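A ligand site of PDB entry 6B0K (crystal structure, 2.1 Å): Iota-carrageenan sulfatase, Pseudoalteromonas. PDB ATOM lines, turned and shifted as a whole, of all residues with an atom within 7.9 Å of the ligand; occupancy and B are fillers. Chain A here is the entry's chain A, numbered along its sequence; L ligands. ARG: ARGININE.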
ATOM      1  N   SER A  37     -16.590 -18.656  -6.754  1.00  0.00           N
ATOM      2  CA  SER A  37     -17.808 -17.985  -7.233  1.00  0.00           C
ATOM      3  C   SER A  37     -18.627 -18.840  -8.236  1.00  0.00           C
ATOM      4  O   SER A  37     -19.491 -18.322  -8.930  1.00  0.00           O
ATOM      5  CB  SER A  37     -17.485 -16.605  -7.820  1.00  0.00           C
ATOM      6  OG  SER A  37     -16.621 -16.696  -8.918  1.00  0.00           O
ATOM      7  N   THR A  39     -19.446 -23.451  -9.254  1.00  0.00           N
ATOM      8  CA  THR A  39     -19.665 -24.783  -8.726  1.00  0.00           C
ATOM      9  C   THR A  39     -18.564 -25.712  -9.253  1.00  0.00           C
ATOM     10  O   THR A  39     -18.334 -25.781 -10.446  1.00  0.00           O
ATOM     11  CB  THR A  39     -21.057 -25.336  -9.109  1.00  0.00           C
ATOM     12  OG1 THR A  39     -22.077 -24.513  -8.547  1.00  0.00           O
ATOM     13  CG2 THR A  39     -21.246 -26.747  -8.593  1.00  0.00           C
ATOM     14  N   TRP A 298     -20.544 -19.170 -14.076  1.00  0.00           N
ATOM     15  CA  TRP A 298     -21.492 -18.365 -14.854  1.00  0.00           C
ATOM     16  C   TRP A 298     -22.411 -17.641 -13.842  1.00  0.00           C
ATOM     17  O   TRP A 298     -23.365 -18.245 -13.348  1.00  0.00           O
ATOM     18  CB  TRP A 298     -22.274 -19.261 -15.823  1.00  0.00           C
ATOM     19  CG  TRP A 298     -23.180 -18.560 -16.800  1.00  0.00           C
ATOM     20  CD1 TRP A 298     -23.118 -17.256 -17.206  1.00  0.00           C
ATOM     21  CD2 TRP A 298     -24.262 -19.145 -17.526  1.00  0.00           C
ATOM     22  NE1 TRP A 298     -24.106 -16.983 -18.106  1.00  0.00           N
ATOM     23  CE2 TRP A 298     -24.841 -18.126 -18.321  1.00  0.00           C
ATOM     24  CE3 TRP A 298     -24.826 -20.425 -17.566  1.00  0.00           C
ATOM     25  CZ2 TRP A 298     -25.951 -18.344 -19.149  1.00  0.00           C
ATOM     26  CZ3 TRP A 298     -25.938 -20.647 -18.380  1.00  0.00           C
ATOM     27  CH2 TRP A 298     -26.482 -19.609 -19.165  1.00  0.00           C
ATOM     28  N   PRO A 299     -22.084 -16.378 -13.494  1.00  0.00           N
ATOM     29  CA  PRO A 299     -22.789 -15.680 -12.400  1.00  0.00           C
ATOM     30  C   PRO A 299     -24.297 -15.574 -12.610  1.00  0.00           C
ATOM     31  O   PRO A 299     -24.764 -15.312 -13.717  1.00  0.00           O
ATOM     32  CB  PRO A 299     -22.153 -14.279 -12.403  1.00  0.00           C
ATOM     33  CG  PRO A 299     -20.829 -14.455 -13.038  1.00  0.00           C
ATOM     34  CD  PRO A 299     -21.005 -15.554 -14.059  1.00  0.00           C
ATOM     35  N   LYS A 300     -25.040 -15.822 -11.527  1.00  0.00           N
ATOM     36  CA  LYS A 300     -26.506 -15.848 -11.509  1.00  0.00           C
ATOM     37  C   LYS A 300     -27.128 -17.129 -12.094  1.00  0.00           C
ATOM     38  O   LYS A 300     -28.317 -17.377 -11.856  1.00  0.00           O
ATOM     39  CB  LYS A 300     -27.121 -14.582 -12.169  1.00  0.00           C
ATOM     40  N   HIS A 301     -26.343 -17.948 -12.804  1.00  0.00           N
ATOM     41  CA  HIS A 301     -26.830 -19.180 -13.429  1.00  0.00           C
ATOM     42  C   HIS A 301     -26.271 -20.413 -12.749  1.00  0.00           C
ATOM     43  O   HIS A 301     -27.025 -21.296 -12.348  1.00  0.00           O
ATOM     44  CB  HIS A 301     -26.489 -19.193 -14.921  1.00  0.00           C
ATOM     45  CG  HIS A 301     -27.134 -18.067 -15.682  1.00  0.00           C
ATOM     46  ND1 HIS A 301     -28.406 -18.156 -16.202  1.00  0.00           N
ATOM     47  CD2 HIS A 301     -26.703 -16.813 -15.956  1.00  0.00           C
ATOM     48  CE1 HIS A 301     -28.720 -17.019 -16.795  1.00  0.00           C
ATOM     49  NE2 HIS A 301     -27.701 -16.183 -16.649  1.00  0.00           N
ATOM     50  N   VAL A 302     -24.936 -20.468 -12.639  1.00  0.00           N
ATOM     51  CA  VAL A 302     -24.254 -21.496 -11.858  1.00  0.00           C
ATOM     52  C   VAL A 302     -24.213 -20.963 -10.439  1.00  0.00           C
ATOM     53  O   VAL A 302     -23.692 -19.873 -10.234  1.00  0.00           O
ATOM     54  CB  VAL A 302     -22.802 -21.723 -12.343  1.00  0.00           C
ATOM     55  CG1 VAL A 302     -22.044 -22.649 -11.396  1.00  0.00           C
ATOM     56  CG2 VAL A 302     -22.799 -22.284 -13.761  1.00  0.00           C
ATOM     57  N   PRO A 303     -24.759 -21.714  -9.454  1.00  0.00           N
ATOM     58  CA  PRO A 303     -24.661 -21.279  -8.061  1.00  0.00           C
ATOM     59  C   PRO A 303     -23.217 -21.082  -7.585  1.00  0.00           C
ATOM     60  O   PRO A 303     -22.334 -21.870  -7.935  1.00  0.00           O
ATOM     61  CB  PRO A 303     -25.296 -22.436  -7.280  1.00  0.00           C
ATOM     62  CG  PRO A 303     -26.224 -23.087  -8.258  1.00  0.00           C
ATOM     63  CD  PRO A 303     -25.551 -22.951  -9.596  1.00  0.00           C
ATOM     64  N   ALA A 304     -22.989 -20.030  -6.785  1.00  0.00           N
ATOM     65  CA  ALA A 304     -21.659 -19.684  -6.297  1.00  0.00           C
ATOM     66  C   ALA A 304     -21.309 -20.411  -4.994  1.00  0.00           C
ATOM     67  O   ALA A 304     -22.159 -20.562  -4.114  1.00  0.00           O
ATOM     68  CB  ALA A 304     -21.570 -18.176  -6.090  1.00  0.00           C
ATOM     69  N   LYS A 306     -20.471 -23.608  -4.425  1.00  0.00           N
ATOM     70  CA  LYS A 306     -21.068 -24.927  -4.251  1.00  0.00           C
ATOM     71  C   LYS A 306     -20.184 -26.031  -4.808  1.00  0.00           C
ATOM     72  O   LYS A 306     -19.298 -25.775  -5.637  1.00  0.00           O
ATOM     73  CB  LYS A 306     -22.442 -24.993  -4.929  1.00  0.00           C
ATOM     74  CG  LYS A 306     -23.413 -23.883  -4.532  1.00  0.00           C
ATOM     75  CD  LYS A 306     -23.613 -23.846  -3.019  1.00  0.00           C
ATOM     76  CE  LYS A 306     -24.645 -22.849  -2.561  1.00  0.00           C
ATOM     77  NZ  LYS A 306     -24.720 -22.893  -1.066  1.00  0.00           N
ATOM     78  N   TRP A 341     -28.058 -29.772 -17.442  1.00  0.00           N
ATOM     79  CA  TRP A 341     -28.508 -28.550 -16.800  1.00  0.00           C
ATOM     80  C   TRP A 341     -29.783 -28.689 -15.931  1.00  0.00           C
ATOM     81  O   TRP A 341     -29.773 -28.246 -14.772  1.00  0.00           O
ATOM     82  CB  TRP A 341     -28.651 -27.414 -17.827  1.00  0.00           C
ATOM     83  CG  TRP A 341     -28.710 -26.082 -17.199  1.00  0.00           C
ATOM     84  CD1 TRP A 341     -29.836 -25.341 -16.966  1.00  0.00           C
ATOM     85  CD2 TRP A 341     -27.617 -25.324 -16.684  1.00  0.00           C
ATOM     86  NE1 TRP A 341     -29.498 -24.158 -16.347  1.00  0.00           N
ATOM     87  CE2 TRP A 341     -28.144 -24.125 -16.163  1.00  0.00           C
ATOM     88  CE3 TRP A 341     -26.230 -25.535 -16.612  1.00  0.00           C
ATOM     89  CZ2 TRP A 341     -27.336 -23.135 -15.580  1.00  0.00           C
ATOM     90  CZ3 TRP A 341     -25.425 -24.558 -16.033  1.00  0.00           C
ATOM     91  CH2 TRP A 341     -25.976 -23.377 -15.535  1.00  0.00           C
ATOM     92  N   PHE A 344     -28.829 -30.579 -12.871  1.00  0.00           N
ATOM     93  CA  PHE A 344     -27.838 -29.744 -12.172  1.00  0.00           C
ATOM     94  C   PHE A 344     -28.508 -28.637 -11.351  1.00  0.00           C
ATOM     95  O   PHE A 344     -28.193 -28.463 -10.169  1.00  0.00           O
ATOM     96  CB  PHE A 344     -26.880 -29.135 -13.185  1.00  0.00           C
ATOM     97  CG  PHE A 344     -25.894 -28.179 -12.594  1.00  0.00           C
ATOM     98  CD1 PHE A 344     -24.942 -28.605 -11.682  1.00  0.00           C
ATOM     99  CD2 PHE A 344     -25.917 -26.827 -12.952  1.00  0.00           C
ATOM    100  CE1 PHE A 344     -24.035 -27.717 -11.126  1.00  0.00           C
ATOM    101  CE2 PHE A 344     -25.007 -25.931 -12.402  1.00  0.00           C
ATOM    102  CZ  PHE A 344     -24.064 -26.386 -11.483  1.00  0.00           C
ATOM    103  N   ILE A 345     -29.437 -27.925 -11.971  1.00  0.00           N
ATOM    104  CA  ILE A 345     -30.195 -26.851 -11.311  1.00  0.00           C
ATOM    105  C   ILE A 345     -31.025 -27.359 -10.123  1.00  0.00           C
ATOM    106  O   ILE A 345     -31.236 -26.603  -9.183  1.00  0.00           O
ATOM    107  CB  ILE A 345     -31.075 -26.082 -12.342  1.00  0.00           C
ATOM    108  CG1 ILE A 345     -30.191 -25.282 -13.312  1.00  0.00           C
ATOM    109  CG2 ILE A 345     -32.068 -25.128 -11.674  1.00  0.00           C
ATOM    110  CD1 ILE A 345     -29.160 -24.364 -12.655  1.00  0.00           C
ATOM    111  N   LYS A 346     -31.486 -28.603 -10.145  1.00  0.00           N
ATOM    112  CA  LYS A 346     -32.258 -29.198  -9.062  1.00  0.00           C
ATOM    113  C   LYS A 346     -31.398 -29.972  -8.050  1.00  0.00           C
ATOM    114  O   LYS A 346     -31.938 -30.630  -7.168  1.00  0.00           O
ATOM    115  CB  LYS A 346     -33.350 -30.115  -9.633  1.00  0.00           C
ATOM    116  CG  LYS A 346     -34.337 -29.384 -10.552  1.00  0.00           C
ATOM    117  CD  LYS A 346     -35.219 -30.339 -11.338  1.00  0.00           C
ATOM    118  CE  LYS A 346     -36.204 -31.043 -10.430  1.00  0.00           C
ATOM    119  NZ  LYS A 346     -37.290 -31.691 -11.200  1.00  0.00           N
HETATM  120  N   ARG L   1     -29.576 -17.109  -9.291  1.00  0.00           N
HETATM  121  CA  ARG L   1     -29.328 -18.407  -8.619  1.00  0.00           C
HETATM  122  C   ARG L   1     -27.900 -18.478  -8.050  1.00  0.00           C
HETATM  123  O   ARG L   1     -26.988 -17.831  -8.519  1.00  0.00           O
HETATM  124  CB  ARG L   1     -29.554 -19.554  -9.607  1.00  0.00           C
HETATM  125  CG  ARG L   1     -29.730 -20.907  -8.953  1.00  0.00           C
HETATM  126  CD  ARG L   1     -29.645 -22.012  -9.989  1.00  0.00           C
HETATM  127  NE  ARG L   1     -30.754 -21.955 -10.948  1.00  0.00           N
HETATM  128  CZ  ARG L   1     -30.697 -21.547 -12.229  1.00  0.00           C
HETATM  129  NH1 ARG L   1     -31.802 -21.573 -12.963  1.00  0.00           N
HETATM  130  NH2 ARG L   1     -29.569 -21.118 -12.782  1.00  0.00           N
HETATM  131  OXT ARG L   1     -27.636 -19.192  -7.088  1.00  0.00           O
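Pro 303 touches the ligand (CA to OXT, 3.8 Å). Ile 345 touches the ligand (CD1 to CZ, 3.2 Å). Hydrophobic or aromatic side chains that line the ligand: Pro 303 and Ile 345. Within 4 Å of the ligand: Lys 300, His 301, Pro 303 and Ile 345.
The backbone carbonyl oxygen of Pro 303 is in hydrogen-bond range of the side-chain hydroxyl of Thr 39 (2.7 Å).
The backbone carbonyl oxygen (O) of His 301 sits at hydrogen-bond distance from a nitrogen (NH2) of the ligand (2.6 Å). O of Lys 300 sits at hydrogen-bond distance from N of the ligand, at 2.9 Å.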
